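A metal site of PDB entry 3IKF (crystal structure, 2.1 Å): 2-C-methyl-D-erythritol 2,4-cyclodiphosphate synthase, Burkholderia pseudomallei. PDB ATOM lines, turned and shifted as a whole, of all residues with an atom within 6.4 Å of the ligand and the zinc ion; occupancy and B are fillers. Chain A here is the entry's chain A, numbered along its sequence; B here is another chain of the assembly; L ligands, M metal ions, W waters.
Merely in contact with the ligand: Val 15 (3.7 Å), Ile 63 (3.5 Å), Phe 67 (3.2 Å), Asp 69 (3.5 Å) and Glu 141 of chain B (3.5 Å).
Within 4 Å of the ligand: Asp 14, Val 15, His 16, His 48, Ile 63, Phe 67, Asp 69, Lys 138 of chain B and Glu 141 of chain B.
The nearest printed residue that does not touch the ligand is Thr 139 of chain B (4.1 Å).
The side-chain carboxylate of Asp 14 is in salt-bridge range of the side-chain amino group of Lys 138 of chain B (3.1 Å).
The backbone carbonyl oxygen (O) of Leu 38 is in hydrogen-bond range of a ring nitrogen (ND1) of His 16, 2.8 Å away.
The side-chain hydroxyl (OG) of Ser 41 lies close to a ring nitrogen (NE2) of His 48 (3.3 Å).
OG of Ser 79 lies within hydrogen-bond range of NE2 of His 48 (2.7 Å).
N of Glu 141 of chain B is in hydrogen-bond range of OG1 of Thr 139 of chain B (3.2 Å).
O of Asp 69 lies close to ND1 of His 40 (3.4 Å).
Within 4 Å of the zinc ion: Asp 14, His 16 and His 48.
The nearest printed residue that does not touch the zinc ion is Val 45 (4.6 Å).
N1 of the ligand binds the zinc ion, at 1.9 Å.
OD2 of Asp 14 is bound to the zinc ion.
The zinc ion is bound by a ring nitrogen (NE2) of His 16 (2.0 Å).
The zinc ion is bound by a ring nitrogen (ND1) of His 48 (2.0 Å).
The zinc ion has four donor atoms within binding distance.
Water W3 lies within hydrogen-bond range of an oxygen (O1) of the ligand, the side-chain amino group (NZ) of Lys 138 of chain B and the backbone NH (N) of Thr 139 of chain B.
Water W4 bridges O of Gly 64 (2.9 Å) and N of Asp 69 (3.0 Å).
NZ of Lys 138 of chain B lies within hydrogen-bond range of O1 of the ligand (2.7 Å).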
ATOM      1  N   ASP A  14      11.681 -18.158   3.472  1.00  0.00           N
ATOM      2  CA  ASP A  14      10.386 -17.580   3.233  1.00  0.00           C
ATOM      3  C   ASP A  14      10.409 -16.047   3.404  1.00  0.00           C
ATOM      4  O   ASP A  14      11.215 -15.518   4.162  1.00  0.00           O
ATOM      5  CB  ASP A  14       9.353 -18.206   4.176  1.00  0.00           C
ATOM      6  CG  ASP A  14       7.924 -18.066   3.656  1.00  0.00           C
ATOM      7  OD1 ASP A  14       7.704 -17.878   2.451  1.00  0.00           O
ATOM      8  OD2 ASP A  14       7.019 -18.125   4.489  1.00  0.00           O
ATOM      9  N   VAL A  15       9.535 -15.337   2.686  1.00  0.00           N
ATOM     10  CA  VAL A  15       9.346 -13.898   2.928  1.00  0.00           C
ATOM     11  C   VAL A  15       7.869 -13.612   2.726  1.00  0.00           C
ATOM     12  O   VAL A  15       7.252 -14.227   1.853  1.00  0.00           O
ATOM     13  CB  VAL A  15      10.245 -13.007   1.983  1.00  0.00           C
ATOM     14  CG1 VAL A  15       9.843 -13.178   0.506  1.00  0.00           C
ATOM     15  CG2 VAL A  15      10.193 -11.522   2.390  1.00  0.00           C
ATOM     16  N   HIS A  16       7.300 -12.751   3.562  1.00  0.00           N
ATOM     17  CA  HIS A  16       5.949 -12.230   3.377  1.00  0.00           C
ATOM     18  C   HIS A  16       5.988 -10.724   3.508  1.00  0.00           C
ATOM     19  O   HIS A  16       6.838 -10.172   4.219  1.00  0.00           O
ATOM     20  CB  HIS A  16       4.971 -12.767   4.433  1.00  0.00           C
ATOM     21  CG  HIS A  16       4.610 -14.209   4.239  1.00  0.00           C
ATOM     22  ND1 HIS A  16       3.456 -14.600   3.593  1.00  0.00           N
ATOM     23  CD2 HIS A  16       5.270 -15.346   4.573  1.00  0.00           C
ATOM     24  CE1 HIS A  16       3.414 -15.926   3.542  1.00  0.00           C
ATOM     25  NE2 HIS A  16       4.511 -16.403   4.120  1.00  0.00           N
ATOM     26  N   LEU A  38       1.328 -10.766   5.372  1.00  0.00           N
ATOM     27  CA  LEU A  38       0.266 -11.045   4.408  1.00  0.00           C
ATOM     28  C   LEU A  38       0.486 -12.381   3.757  1.00  0.00           C
ATOM     29  O   LEU A  38       1.537 -12.621   3.155  1.00  0.00           O
ATOM     30  CB  LEU A  38       0.215  -9.955   3.337  1.00  0.00           C
ATOM     31  CG  LEU A  38      -0.731 -10.257   2.158  1.00  0.00           C
ATOM     32  CD1 LEU A  38      -2.198 -10.105   2.608  1.00  0.00           C
ATOM     33  CD2 LEU A  38      -0.421  -9.343   0.941  1.00  0.00           C
ATOM     34  N   HIS A  40      -1.967 -16.265   2.454  1.00  0.00           N
ATOM     35  CA  HIS A  40      -3.162 -17.127   2.435  1.00  0.00           C
ATOM     36  C   HIS A  40      -3.480 -17.774   3.808  1.00  0.00           C
ATOM     37  O   HIS A  40      -4.629 -17.700   4.282  1.00  0.00           O
ATOM     38  CB  HIS A  40      -2.951 -18.204   1.374  1.00  0.00           C
ATOM     39  CG  HIS A  40      -4.125 -19.096   1.142  1.00  0.00           C
ATOM     40  ND1 HIS A  40      -5.298 -18.648   0.577  1.00  0.00           N
ATOM     41  CD2 HIS A  40      -4.280 -20.425   1.332  1.00  0.00           C
ATOM     42  CE1 HIS A  40      -6.147 -19.654   0.463  1.00  0.00           C
ATOM     43  NE2 HIS A  40      -5.560 -20.753   0.911  1.00  0.00           N
ATOM     44  N   SER A  41      -2.461 -18.380   4.424  1.00  0.00           N
ATOM     45  CA  SER A  41      -2.557 -18.916   5.787  1.00  0.00           C
ATOM     46  C   SER A  41      -2.290 -17.765   6.756  1.00  0.00           C
ATOM     47  O   SER A  41      -2.357 -16.596   6.336  1.00  0.00           O
ATOM     48  CB  SER A  41      -1.532 -20.047   6.005  1.00  0.00           C
ATOM     49  OG  SER A  41      -0.190 -19.580   5.962  1.00  0.00           O
ATOM     50  N   ALA A  43       0.350 -16.754   7.565  1.00  0.00           N
ATOM     51  CA  ALA A  43       1.535 -16.076   6.983  1.00  0.00           C
ATOM     52  C   ALA A  43       2.791 -16.092   7.887  1.00  0.00           C
ATOM     53  O   ALA A  43       3.699 -15.245   7.761  1.00  0.00           O
ATOM     54  CB  ALA A  43       1.193 -14.628   6.501  1.00  0.00           C
ATOM     55  N   ASP A  44       2.862 -17.091   8.753  1.00  0.00           N
ATOM     56  CA  ASP A  44       3.956 -17.211   9.712  1.00  0.00           C
ATOM     57  C   ASP A  44       5.241 -17.587   8.992  1.00  0.00           C
ATOM     58  O   ASP A  44       5.506 -18.769   8.729  1.00  0.00           O
ATOM     59  CB  ASP A  44       3.569 -18.255  10.782  1.00  0.00           C
ATOM     60  CG  ASP A  44       4.508 -18.234  11.988  1.00  0.00           C
ATOM     61  OD1 ASP A  44       5.717 -17.997  11.808  1.00  0.00           O
ATOM     62  OD2 ASP A  44       4.027 -18.492  13.109  1.00  0.00           O
ATOM     63  N   VAL A  45       6.029 -16.569   8.654  1.00  0.00           N
ATOM     64  CA  VAL A  45       7.205 -16.739   7.784  1.00  0.00           C
ATOM     65  C   VAL A  45       8.271 -17.693   8.388  1.00  0.00           C
ATOM     66  O   VAL A  45       8.924 -18.451   7.669  1.00  0.00           O
ATOM     67  CB  VAL A  45       7.800 -15.335   7.393  1.00  0.00           C
ATOM     68  CG1 VAL A  45       8.300 -14.554   8.640  1.00  0.00           C
ATOM     69  CG2 VAL A  45       8.894 -15.442   6.365  1.00  0.00           C
ATOM     70  N   HIS A  48       7.033 -21.405   8.224  1.00  0.00           N
ATOM     71  CA  HIS A  48       7.049 -21.881   6.854  1.00  0.00           C
ATOM     72  C   HIS A  48       8.461 -22.254   6.406  1.00  0.00           C
ATOM     73  O   HIS A  48       8.671 -23.260   5.733  1.00  0.00           O
ATOM     74  CB  HIS A  48       6.469 -20.795   5.891  1.00  0.00           C
ATOM     75  CG  HIS A  48       5.007 -20.525   6.106  1.00  0.00           C
ATOM     76  ND1 HIS A  48       4.325 -19.525   5.446  1.00  0.00           N
ATOM     77  CD2 HIS A  48       4.104 -21.130   6.927  1.00  0.00           C
ATOM     78  CE1 HIS A  48       3.061 -19.520   5.852  1.00  0.00           C
ATOM     79  NE2 HIS A  48       2.910 -20.476   6.763  1.00  0.00           N
ATOM     80  N   ALA A  49       9.415 -21.391   6.774  1.00  0.00           N
ATOM     81  CA  ALA A  49      10.812 -21.624   6.475  1.00  0.00           C
ATOM     82  C   ALA A  49      11.304 -22.927   7.168  1.00  0.00           C
ATOM     83  O   ALA A  49      12.018 -23.746   6.546  1.00  0.00           O
ATOM     84  CB  ALA A  49      11.658 -20.383   6.916  1.00  0.00           C
ATOM     85  N   ILE A  63       6.666 -26.886   1.093  1.00  0.00           N
ATOM     86  CA  ILE A  63       5.461 -26.500   1.811  1.00  0.00           C
ATOM     87  C   ILE A  63       4.403 -25.974   0.821  1.00  0.00           C
ATOM     88  O   ILE A  63       3.204 -26.150   1.036  1.00  0.00           O
ATOM     89  CB  ILE A  63       5.765 -25.389   2.852  1.00  0.00           C
ATOM     90  CG1 ILE A  63       4.593 -25.215   3.814  1.00  0.00           C
ATOM     91  CG2 ILE A  63       6.202 -24.061   2.139  1.00  0.00           C
ATOM     92  CD1 ILE A  63       4.826 -24.128   4.889  1.00  0.00           C
ATOM     93  N   GLY A  64       4.859 -25.327  -0.254  1.00  0.00           N
ATOM     94  CA  GLY A  64       3.949 -24.801  -1.283  1.00  0.00           C
ATOM     95  C   GLY A  64       3.134 -25.905  -1.920  1.00  0.00           C
ATOM     96  O   GLY A  64       2.008 -25.676  -2.364  1.00  0.00           O
ATOM     97  N   ARG A  65       3.686 -27.119  -1.907  1.00  0.00           N
ATOM     98  CA  ARG A  65       3.049 -28.315  -2.446  1.00  0.00           C
ATOM     99  C   ARG A  65       2.196 -29.112  -1.440  1.00  0.00           C
ATOM    100  O   ARG A  65       1.086 -29.559  -1.771  1.00  0.00           O
ATOM    101  CB  ARG A  65       4.144 -29.224  -2.986  1.00  0.00           C
ATOM    102  CG  ARG A  65       3.741 -30.661  -3.185  1.00  0.00           C
ATOM    103  CD  ARG A  65       4.990 -31.505  -3.185  1.00  0.00           C
ATOM    104  NE  ARG A  65       4.726 -32.904  -2.865  1.00  0.00           N
ATOM    105  CZ  ARG A  65       5.553 -33.904  -3.164  1.00  0.00           C
ATOM    106  NH1 ARG A  65       5.253 -35.161  -2.825  1.00  0.00           N
ATOM    107  NH2 ARG A  65       6.676 -33.651  -3.824  1.00  0.00           N
ATOM    108  N   PHE A  67       0.995 -27.900   1.337  1.00  0.00           N
ATOM    109  CA  PHE A  67       0.005 -26.983   1.911  1.00  0.00           C
ATOM    110  C   PHE A  67      -0.185 -25.741   1.012  1.00  0.00           C
ATOM    111  O   PHE A  67       0.174 -24.592   1.369  1.00  0.00           O
ATOM    112  CB  PHE A  67       0.420 -26.570   3.338  1.00  0.00           C
ATOM    113  CG  PHE A  67       0.811 -27.735   4.247  1.00  0.00           C
ATOM    114  CD1 PHE A  67      -0.042 -28.817   4.457  1.00  0.00           C
ATOM    115  CD2 PHE A  67       2.031 -27.716   4.931  1.00  0.00           C
ATOM    116  CE1 PHE A  67       0.344 -29.884   5.319  1.00  0.00           C
ATOM    117  CE2 PHE A  67       2.417 -28.783   5.794  1.00  0.00           C
ATOM    118  CZ  PHE A  67       1.570 -29.841   5.989  1.00  0.00           C
ATOM    119  N   SER A  68      -0.765 -25.977  -0.166  1.00  0.00           N
ATOM    120  CA  SER A  68      -0.832 -24.960  -1.241  1.00  0.00           C
ATOM    121  C   SER A  68      -1.528 -23.635  -0.884  1.00  0.00           C
ATOM    122  O   SER A  68      -2.572 -23.636  -0.209  1.00  0.00           O
ATOM    123  CB  SER A  68      -1.443 -25.594  -2.498  1.00  0.00           C
ATOM    124  OG  SER A  68      -1.730 -24.613  -3.491  1.00  0.00           O
ATOM    125  N   ASP A  69      -0.966 -22.513  -1.329  1.00  0.00           N
ATOM    126  CA  ASP A  69      -1.581 -21.217  -1.080  1.00  0.00           C
ATOM    127  C   ASP A  69      -2.756 -20.962  -2.018  1.00  0.00           C
ATOM    128  O   ASP A  69      -3.413 -19.933  -1.927  1.00  0.00           O
ATOM    129  CB  ASP A  69      -0.584 -20.045  -1.092  1.00  0.00           C
ATOM    130  CG  ASP A  69       0.215 -19.929  -2.383  1.00  0.00           C
ATOM    131  OD1 ASP A  69      -0.109 -20.579  -3.408  1.00  0.00           O
ATOM    132  OD2 ASP A  69       1.204 -19.168  -2.361  1.00  0.00           O
ATOM    133  N   SER A  79      -0.204 -22.068  11.123  1.00  0.00           N
ATOM    134  CA  SER A  79       1.050 -22.624  10.625  1.00  0.00           C
ATOM    135  C   SER A  79       1.759 -23.550  11.617  1.00  0.00           C
ATOM    136  O   SER A  79       2.669 -24.301  11.231  1.00  0.00           O
ATOM    137  CB  SER A  79       1.997 -21.503  10.187  1.00  0.00           C
ATOM    138  OG  SER A  79       1.490 -20.850   9.019  1.00  0.00           O
ATOM    139  N   LEU A  82       0.273 -26.730  10.601  1.00  0.00           N
ATOM    140  CA  LEU A  82       0.989 -27.113   9.394  1.00  0.00           C
ATOM    141  C   LEU A  82       2.373 -27.709   9.717  1.00  0.00           C
ATOM    142  O   LEU A  82       2.750 -28.745   9.187  1.00  0.00           O
ATOM    143  CB  LEU A  82       1.095 -25.920   8.432  1.00  0.00           C
ATOM    144  CG  LEU A  82      -0.205 -25.310   7.835  1.00  0.00           C
ATOM    145  CD1 LEU A  82       0.146 -24.315   6.712  1.00  0.00           C
ATOM    146  CD2 LEU A  82      -1.158 -26.374   7.308  1.00  0.00           C
ATOM    147  N   LYS B 138       9.879 -21.300  -4.580  1.00  0.00           N
ATOM    148  CA  LYS B 138       9.296 -20.141  -3.875  1.00  0.00           C
ATOM    149  C   LYS B 138       9.127 -18.960  -4.830  1.00  0.00           C
ATOM    150  O   LYS B 138       9.826 -18.864  -5.834  1.00  0.00           O
ATOM    151  CB  LYS B 138      10.215 -19.686  -2.742  1.00  0.00           C
ATOM    152  CG  LYS B 138      10.513 -20.719  -1.636  1.00  0.00           C
ATOM    153  CD  LYS B 138       9.249 -21.164  -0.881  1.00  0.00           C
ATOM    154  CE  LYS B 138       8.729 -20.149   0.134  1.00  0.00           C
ATOM    155  NZ  LYS B 138       8.126 -18.895  -0.395  1.00  0.00           N
ATOM    156  N   THR B 139       8.221 -18.053  -4.502  1.00  0.00           N
ATOM    157  CA  THR B 139       8.191 -16.750  -5.105  1.00  0.00           C
ATOM    158  C   THR B 139       8.730 -15.774  -4.066  1.00  0.00           C
ATOM    159  O   THR B 139       8.925 -16.149  -2.891  1.00  0.00           O
ATOM    160  CB  THR B 139       6.761 -16.296  -5.544  1.00  0.00           C
ATOM    161  OG1 THR B 139       6.046 -15.784  -4.414  1.00  0.00           O
ATOM    162  CG2 THR B 139       5.962 -17.443  -6.178  1.00  0.00           C
ATOM    163  N   ASN B 140       8.957 -14.528  -4.460  1.00  0.00           N
ATOM    164  CA  ASN B 140       9.408 -13.561  -3.478  1.00  0.00           C
ATOM    165  C   ASN B 140       8.308 -12.656  -2.960  1.00  0.00           C
ATOM    166  O   ASN B 140       8.591 -11.603  -2.351  1.00  0.00           O
ATOM    167  CB  ASN B 140      10.622 -12.774  -3.950  1.00  0.00           C
ATOM    168  CG  ASN B 140      11.603 -12.540  -2.834  1.00  0.00           C
ATOM    169  OD1 ASN B 140      12.018 -13.483  -2.161  1.00  0.00           O
ATOM    170  ND2 ASN B 140      11.961 -11.264  -2.599  1.00  0.00           N
ATOM    171  N   GLU B 141       7.072 -13.072  -3.164  1.00  0.00           N
ATOM    172  CA  GLU B 141       5.914 -12.306  -2.717  1.00  0.00           C
ATOM    173  C   GLU B 141       5.969 -10.846  -3.211  1.00  0.00           C
ATOM    174  O   GLU B 141       5.573  -9.916  -2.501  1.00  0.00           O
ATOM    175  CB  GLU B 141       5.742 -12.405  -1.186  1.00  0.00           C
ATOM    176  CG  GLU B 141       5.299 -13.775  -0.717  1.00  0.00           C
ATOM    177  CD  GLU B 141       3.863 -14.092  -1.140  1.00  0.00           C
ATOM    178  OE1 GLU B 141       2.951 -13.343  -0.730  1.00  0.00           O
ATOM    179  OE2 GLU B 141       3.645 -15.077  -1.868  1.00  0.00           O
HETATM  180  C1  LIG L   1       4.448 -18.447   1.141  1.00  0.00           C
HETATM  181  N1  LIG L   1       4.549 -19.096   2.359  1.00  0.00           N
HETATM  182  C2  LIG L   1       3.770 -20.206   2.146  1.00  0.00           C
HETATM  183  N2  LIG L   1       3.230 -20.262   0.921  1.00  0.00           N
HETATM  184  C3  LIG L   1       3.642 -19.142   0.214  1.00  0.00           C
HETATM  185  C4  LIG L   1       2.413 -21.361   0.618  1.00  0.00           C
HETATM  186  C5  LIG L   1       2.349 -22.223   1.745  1.00  0.00           C
HETATM  187  S1  LIG L   1       3.303 -21.537   3.057  1.00  0.00           S
HETATM  188  C6  LIG L   1       5.143 -17.148   0.842  1.00  0.00           C
HETATM  189  O1  LIG L   1       5.878 -17.365  -0.359  1.00  0.00           O
HETATM  190 ZN    ZN M   1       5.131 -18.329   4.002  1.00  0.00          ZN
HETATM  191  O   HOH W   1       5.910 -21.939  -0.348  1.00  0.00           O
HETATM  192  O   HOH W   2      -0.928 -21.920   2.140  1.00  0.00           O
HETATM  193  O   HOH W   3       6.199 -18.961  -2.411  1.00  0.00           O
HETATM  194  O   HOH W   4       1.751 -22.771  -2.486  1.00  0.00           O
HETATM  195  O   HOH W   5       8.104 -16.092  -0.166  1.00  0.00           O
